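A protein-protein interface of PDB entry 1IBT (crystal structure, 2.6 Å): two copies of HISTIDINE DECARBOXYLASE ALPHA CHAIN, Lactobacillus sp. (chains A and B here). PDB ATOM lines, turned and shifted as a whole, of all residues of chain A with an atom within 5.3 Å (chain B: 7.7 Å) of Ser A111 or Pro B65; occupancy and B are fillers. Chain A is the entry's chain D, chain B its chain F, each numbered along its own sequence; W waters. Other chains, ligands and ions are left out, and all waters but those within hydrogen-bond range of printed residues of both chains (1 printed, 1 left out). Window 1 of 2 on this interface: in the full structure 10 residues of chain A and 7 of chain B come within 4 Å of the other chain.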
ATOM      1  N   PHE A   2     -17.477  18.780 -15.453  1.00  0.00           N
ATOM      2  CA  PHE A   2     -16.650  19.848 -16.023  1.00  0.00           C
ATOM      3  C   PHE A   2     -17.009  21.270 -15.568  1.00  0.00           C
ATOM      4  O   PHE A   2     -18.042  21.493 -14.931  1.00  0.00           O
ATOM      5  CB  PHE A   2     -16.740  19.776 -17.519  1.00  0.00           C
ATOM      6  CG  PHE A   2     -16.273  18.427 -18.035  1.00  0.00           C
ATOM      7  CD1 PHE A   2     -14.922  18.188 -18.285  1.00  0.00           C
ATOM      8  CD2 PHE A   2     -17.208  17.402 -18.231  1.00  0.00           C
ATOM      9  CE1 PHE A   2     -14.522  16.927 -18.727  1.00  0.00           C
ATOM     10  CE2 PHE A   2     -16.794  16.144 -18.669  1.00  0.00           C
ATOM     11  CZ  PHE A   2     -15.451  15.906 -18.918  1.00  0.00           C
ATOM     12  N   THR A   3     -16.076  22.203 -15.772  1.00  0.00           N
ATOM     13  CA  THR A   3     -16.268  23.636 -15.594  1.00  0.00           C
ATOM     14  C   THR A   3     -15.619  24.232 -16.833  1.00  0.00           C
ATOM     15  O   THR A   3     -14.384  24.184 -16.960  1.00  0.00           O
ATOM     16  CB  THR A   3     -15.529  24.178 -14.395  1.00  0.00           C
ATOM     17  OG1 THR A   3     -16.008  23.415 -13.315  1.00  0.00           O
ATOM     18  CG2 THR A   3     -15.697  25.676 -14.188  1.00  0.00           C
ATOM     19  N   GLY A   4     -16.408  24.759 -17.757  1.00  0.00           N
ATOM     20  CA  GLY A   4     -15.859  25.259 -18.994  1.00  0.00           C
ATOM     21  C   GLY A   4     -15.885  26.758 -19.094  1.00  0.00           C
ATOM     22  O   GLY A   4     -15.655  27.494 -18.138  1.00  0.00           O
ATOM     23  N   VAL A   5     -16.269  27.210 -20.272  1.00  0.00           N
ATOM     24  CA  VAL A   5     -16.237  28.610 -20.601  1.00  0.00           C
ATOM     25  C   VAL A   5     -17.147  29.431 -19.713  1.00  0.00           C
ATOM     26  O   VAL A   5     -16.973  30.644 -19.610  1.00  0.00           O
ATOM     27  CB  VAL A   5     -16.613  28.802 -22.076  1.00  0.00           C
ATOM     28  CG1 VAL A   5     -15.500  28.184 -22.828  1.00  0.00           C
ATOM     29  CG2 VAL A   5     -17.880  28.132 -22.525  1.00  0.00           C
ATOM     30  N   GLN A   6     -18.095  28.851 -19.004  1.00  0.00           N
ATOM     31  CA  GLN A   6     -18.966  29.663 -18.210  1.00  0.00           C
ATOM     32  C   GLN A   6     -18.566  29.696 -16.780  1.00  0.00           C
ATOM     33  O   GLN A   6     -19.336  30.304 -16.020  1.00  0.00           O
ATOM     34  CB  GLN A   6     -20.337  29.142 -18.250  1.00  0.00           C
ATOM     35  CG  GLN A   6     -20.875  29.116 -19.597  1.00  0.00           C
ATOM     36  CD  GLN A   6     -21.912  28.063 -19.611  1.00  0.00           C
ATOM     37  OE1 GLN A   6     -21.628  26.977 -20.109  1.00  0.00           O
ATOM     38  NE2 GLN A   6     -23.091  28.293 -19.063  1.00  0.00           N
ATOM     39  N   SER A 102      -8.938  19.961 -12.499  1.00  0.00           N
ATOM     40  CA  SER A 102      -7.794  20.106 -13.352  1.00  0.00           C
ATOM     41  C   SER A 102      -8.136  21.284 -14.242  1.00  0.00           C
ATOM     42  O   SER A 102      -9.093  21.252 -15.025  1.00  0.00           O
ATOM     43  CB  SER A 102      -7.654  18.808 -14.112  1.00  0.00           C
ATOM     44  OG  SER A 102      -7.839  17.701 -13.249  1.00  0.00           O
ATOM     45  N   ALA A 104      -8.030  23.797 -17.151  1.00  0.00           N
ATOM     46  CA  ALA A 104      -7.597  23.736 -18.530  1.00  0.00           C
ATOM     47  C   ALA A 104      -6.564  24.817 -18.814  1.00  0.00           C
ATOM     48  O   ALA A 104      -6.552  25.907 -18.226  1.00  0.00           O
ATOM     49  CB  ALA A 104      -8.786  23.904 -19.460  1.00  0.00           C
ATOM     50  N   THR A 108     -10.580  28.735 -23.238  1.00  0.00           N
ATOM     51  CA  THR A 108     -11.364  29.209 -24.338  1.00  0.00           C
ATOM     52  C   THR A 108     -11.649  28.026 -25.227  1.00  0.00           C
ATOM     53  O   THR A 108     -12.730  27.943 -25.822  1.00  0.00           O
ATOM     54  CB  THR A 108     -10.500  30.273 -24.937  1.00  0.00           C
ATOM     55  OG1 THR A 108     -10.416  31.253 -23.897  1.00  0.00           O
ATOM     56  CG2 THR A 108     -10.963  30.762 -26.283  1.00  0.00           C
ATOM     57  N   LYS A 109     -10.690  27.118 -25.356  1.00  0.00           N
ATOM     58  CA  LYS A 109     -10.915  25.967 -26.200  1.00  0.00           C
ATOM     59  C   LYS A 109     -11.388  24.752 -25.366  1.00  0.00           C
ATOM     60  O   LYS A 109     -12.288  24.001 -25.778  1.00  0.00           O
ATOM     61  CB  LYS A 109      -9.572  25.737 -26.970  1.00  0.00           C
ATOM     62  CG  LYS A 109      -9.330  24.421 -27.769  1.00  0.00           C
ATOM     63  CD  LYS A 109      -7.795  24.175 -27.858  1.00  0.00           C
ATOM     64  CE  LYS A 109      -7.381  22.719 -28.177  1.00  0.00           C
ATOM     65  NZ  LYS A 109      -7.668  21.839 -27.051  1.00  0.00           N
ATOM     66  N   ASP A 110     -10.824  24.590 -24.171  1.00  0.00           N
ATOM     67  CA  ASP A 110     -11.024  23.395 -23.379  1.00  0.00           C
ATOM     68  C   ASP A 110     -11.659  23.620 -22.025  1.00  0.00           C
ATOM     69  O   ASP A 110     -11.461  24.659 -21.407  1.00  0.00           O
ATOM     70  CB  ASP A 110      -9.679  22.683 -23.114  1.00  0.00           C
ATOM     71  CG  ASP A 110      -8.897  22.207 -24.318  1.00  0.00           C
ATOM     72  OD1 ASP A 110      -9.471  21.559 -25.205  1.00  0.00           O
ATOM     73  OD2 ASP A 110      -7.701  22.505 -24.408  1.00  0.00           O
ATOM     74  N   SER A 111     -12.333  22.612 -21.504  1.00  0.00           N
ATOM     75  CA  SER A 111     -12.933  22.693 -20.208  1.00  0.00           C
ATOM     76  C   SER A 111     -11.991  22.193 -19.136  1.00  0.00           C
ATOM     77  O   SER A 111     -11.096  21.377 -19.351  1.00  0.00           O
ATOM     78  CB  SER A 111     -14.196  21.867 -20.196  1.00  0.00           C
ATOM     79  OG  SER A 111     -14.999  22.008 -19.020  1.00  0.00           O
ATOM     80  N   SER A 112     -12.141  22.747 -17.941  1.00  0.00           N
ATOM     81  CA  SER A 112     -11.476  22.222 -16.778  1.00  0.00           C
ATOM     82  C   SER A 112     -12.319  21.044 -16.366  1.00  0.00           C
ATOM     83  O   SER A 112     -13.525  20.999 -16.645  1.00  0.00           O
ATOM     84  CB  SER A 112     -11.478  23.235 -15.716  1.00  0.00           C
ATOM     85  OG  SER A 112     -10.644  24.271 -16.166  1.00  0.00           O
ATOM     86  N   MET A 113     -11.720  20.091 -15.677  1.00  0.00           N
ATOM     87  CA  MET A 113     -12.399  18.851 -15.339  1.00  0.00           C
ATOM     88  C   MET A 113     -12.292  18.576 -13.862  1.00  0.00           C
ATOM     89  O   MET A 113     -11.325  18.970 -13.216  1.00  0.00           O
ATOM     90  CB  MET A 113     -11.759  17.713 -16.130  1.00  0.00           C
ATOM     91  CG  MET A 113     -12.378  16.317 -16.021  1.00  0.00           C
ATOM     92  SD  MET A 113     -11.454  15.157 -17.043  1.00  0.00           S
ATOM     93  CE  MET A 113      -9.918  15.252 -16.187  1.00  0.00           C
ATOM     94  N   ALA A 153      -7.036  17.954 -24.376  1.00  0.00           N
ATOM     95  CA  ALA A 153      -7.162  19.004 -23.397  1.00  0.00           C
ATOM     96  C   ALA A 153      -5.984  18.975 -22.460  1.00  0.00           C
ATOM     97  O   ALA A 153      -5.996  18.172 -21.541  1.00  0.00           O
ATOM     98  CB  ALA A 153      -8.446  18.799 -22.595  1.00  0.00           C
ATOM     99  N   PHE A 155      -3.939  20.258 -19.317  1.00  0.00           N
ATOM    100  CA  PHE A 155      -4.330  21.054 -18.160  1.00  0.00           C
ATOM    101  C   PHE A 155      -3.114  21.783 -17.667  1.00  0.00           C
ATOM    102  O   PHE A 155      -2.037  21.542 -18.207  1.00  0.00           O
ATOM    103  CB  PHE A 155      -4.873  20.161 -17.063  1.00  0.00           C
ATOM    104  CG  PHE A 155      -6.099  19.367 -17.501  1.00  0.00           C
ATOM    105  CD1 PHE A 155      -7.350  19.961 -17.513  1.00  0.00           C
ATOM    106  CD2 PHE A 155      -5.967  18.032 -17.900  1.00  0.00           C
ATOM    107  CE1 PHE A 155      -8.466  19.223 -17.923  1.00  0.00           C
ATOM    108  CE2 PHE A 155      -7.087  17.306 -18.306  1.00  0.00           C
ATOM    109  CZ  PHE A 155      -8.341  17.892 -18.321  1.00  0.00           C
ATOM    110  N   ARG B  59     -14.073  18.824 -35.178  1.00  0.00           N
ATOM    111  CA  ARG B  59     -15.049  19.406 -34.258  1.00  0.00           C
ATOM    112  C   ARG B  59     -15.938  20.440 -34.944  1.00  0.00           C
ATOM    113  O   ARG B  59     -15.419  21.411 -35.497  1.00  0.00           O
ATOM    114  CB  ARG B  59     -14.264  20.013 -33.096  1.00  0.00           C
ATOM    115  CG  ARG B  59     -13.900  19.088 -31.938  1.00  0.00           C
ATOM    116  CD  ARG B  59     -12.864  19.881 -31.185  1.00  0.00           C
ATOM    117  NE  ARG B  59     -12.657  19.649 -29.743  1.00  0.00           N
ATOM    118  CZ  ARG B  59     -11.833  18.712 -29.246  1.00  0.00           C
ATOM    119  NH1 ARG B  59     -11.169  17.891 -30.063  1.00  0.00           N
ATOM    120  NH2 ARG B  59     -11.561  18.687 -27.937  1.00  0.00           N
ATOM    121  N   TYR B  62     -20.481  21.159 -31.697  1.00  0.00           N
ATOM    122  CA  TYR B  62     -20.580  20.271 -30.558  1.00  0.00           C
ATOM    123  C   TYR B  62     -20.975  21.038 -29.316  1.00  0.00           C
ATOM    124  O   TYR B  62     -21.014  22.261 -29.376  1.00  0.00           O
ATOM    125  CB  TYR B  62     -19.254  19.586 -30.370  1.00  0.00           C
ATOM    126  CG  TYR B  62     -18.097  20.464 -30.042  1.00  0.00           C
ATOM    127  CD1 TYR B  62     -17.344  21.018 -31.047  1.00  0.00           C
ATOM    128  CD2 TYR B  62     -17.761  20.682 -28.729  1.00  0.00           C
ATOM    129  CE1 TYR B  62     -16.239  21.797 -30.731  1.00  0.00           C
ATOM    130  CE2 TYR B  62     -16.652  21.458 -28.404  1.00  0.00           C
ATOM    131  CZ  TYR B  62     -15.905  22.007 -29.419  1.00  0.00           C
ATOM    132  OH  TYR B  62     -14.824  22.777 -29.138  1.00  0.00           O
ATOM    133  N   PRO B  63     -21.302  20.466 -28.174  1.00  0.00           N
ATOM    134  CA  PRO B  63     -21.668  21.253 -27.033  1.00  0.00           C
ATOM    135  C   PRO B  63     -20.505  21.982 -26.392  1.00  0.00           C
ATOM    136  O   PRO B  63     -19.359  21.549 -26.400  1.00  0.00           O
ATOM    137  CB  PRO B  63     -22.359  20.239 -26.187  1.00  0.00           C
ATOM    138  CG  PRO B  63     -23.030  19.339 -27.170  1.00  0.00           C
ATOM    139  CD  PRO B  63     -21.835  19.122 -28.036  1.00  0.00           C
ATOM    140  N   ALA B  64     -20.834  23.155 -25.887  1.00  0.00           N
ATOM    141  CA  ALA B  64     -19.895  24.055 -25.273  1.00  0.00           C
ATOM    142  C   ALA B  64     -19.102  23.454 -24.136  1.00  0.00           C
ATOM    143  O   ALA B  64     -19.697  22.808 -23.284  1.00  0.00           O
ATOM    144  CB  ALA B  64     -20.671  25.257 -24.772  1.00  0.00           C
ATOM    145  N   PRO B  65     -17.806  23.652 -23.998  1.00  0.00           N
ATOM    146  CA  PRO B  65     -17.013  23.176 -22.885  1.00  0.00           C
ATOM    147  C   PRO B  65     -17.634  23.455 -21.530  1.00  0.00           C
ATOM    148  O   PRO B  65     -17.744  24.628 -21.192  1.00  0.00           O
ATOM    149  CB  PRO B  65     -15.690  23.861 -23.096  1.00  0.00           C
ATOM    150  CG  PRO B  65     -15.556  23.894 -24.577  1.00  0.00           C
ATOM    151  CD  PRO B  65     -16.959  24.311 -24.959  1.00  0.00           C
ATOM    152  N   GLY B  66     -18.082  22.488 -20.746  1.00  0.00           N
ATOM    153  CA  GLY B  66     -18.640  22.740 -19.428  1.00  0.00           C
ATOM    154  C   GLY B  66     -20.123  23.071 -19.457  1.00  0.00           C
ATOM    155  O   GLY B  66     -20.672  23.501 -18.449  1.00  0.00           O
ATOM    156  N   SER B  67     -20.781  22.938 -20.601  1.00  0.00           N
ATOM    157  CA  SER B  67     -22.183  23.251 -20.718  1.00  0.00           C
ATOM    158  C   SER B  67     -23.018  22.211 -20.017  1.00  0.00           C
ATOM    159  O   SER B  67     -22.509  21.131 -19.747  1.00  0.00           O
ATOM    160  CB  SER B  67     -22.579  23.272 -22.146  1.00  0.00           C
ATOM    161  OG  SER B  67     -22.252  22.076 -22.858  1.00  0.00           O
ATOM    162  N   PHE B  68     -24.288  22.397 -19.725  1.00  0.00           N
ATOM    163  CA  PHE B  68     -25.037  21.400 -19.031  1.00  0.00           C
ATOM    164  C   PHE B  68     -26.036  20.859 -20.000  1.00  0.00           C
ATOM    165  O   PHE B  68     -27.090  21.436 -20.232  1.00  0.00           O
ATOM    166  CB  PHE B  68     -25.702  22.035 -17.799  1.00  0.00           C
ATOM    167  CG  PHE B  68     -24.765  22.232 -16.603  1.00  0.00           C
ATOM    168  CD1 PHE B  68     -23.669  23.078 -16.670  1.00  0.00           C
ATOM    169  CD2 PHE B  68     -24.989  21.515 -15.439  1.00  0.00           C
ATOM    170  CE1 PHE B  68     -22.807  23.199 -15.596  1.00  0.00           C
ATOM    171  CE2 PHE B  68     -24.121  21.649 -14.376  1.00  0.00           C
ATOM    172  CZ  PHE B  68     -23.032  22.487 -14.451  1.00  0.00           C
HETATM  173  O   HOH W   1     -13.854  22.356 -26.781  1.00  0.00           O
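Water W1 lies within hydrogen-bond range of the backbone carbonyl oxygen of Lys A109 and the side-chain hydroxyl of Tyr B62.
Hydrophobic or aromatic side chains of chain A within 4 Å of the printed part of chain B: Val A5. Hydrophobic or aromatic side chains of chain B within 4 Å of the printed part of chain A: Pro B65. Among the printed residues, 8 pairs touch across the chains.
N of Val A5 sits at hydrogen-bond distance from O of Pro B65.
Printed residues of chain B within 4 Å of Gln A6: Gly B66 (3.97 Å) and Ser B67 (3.8 Å). Of the printed residues of chain B, Ser A111 touches Pro B65 and Gly B66. Ser A112 touches none of the printed residues of chain B. Of chain A, only Gly A4, Val A5, Lys A109 and Ser A111 come within 4 Å of Pro B65. Of the printed residues of chain A, Ser B67 touches Gln A6. The nearest residue of chain B that does not touch Ser A111 is Ser B67 (6.1 Å). The nearest residue of chain A that does not touch Pro B65 is Asp A110 (4.2 Å).
Pro B65 touches Gly A4 (O to CA, 3.0 Å). Gly A4 touches Gly B66. Gly B66 touches Gln A6 (O to OE1, 3.97 Å). Gln A6 touches Ser B67. Lys A109 touches Pro B65. CB of Ser A111 touches CB of Pro B65, at 3.8 Å. Ser A111 touches Gly B66.
No position is printed for both chains.
O of Thr A3 lies within hydrogen-bond range of OG of Ser A111 (3.1 Å). The side-chain amino group (NZ) of Lys A109 lies within salt-bridge range of the side-chain carboxylate (OD1) of Asp A110. OG of Ser A111 sits at hydrogen-bond distance from N of Gly A4, at 3.3 Å. The backbone carbonyl oxygen of Ala B64 sits at hydrogen-bond distance from the side-chain hydroxyl of Ser B67.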
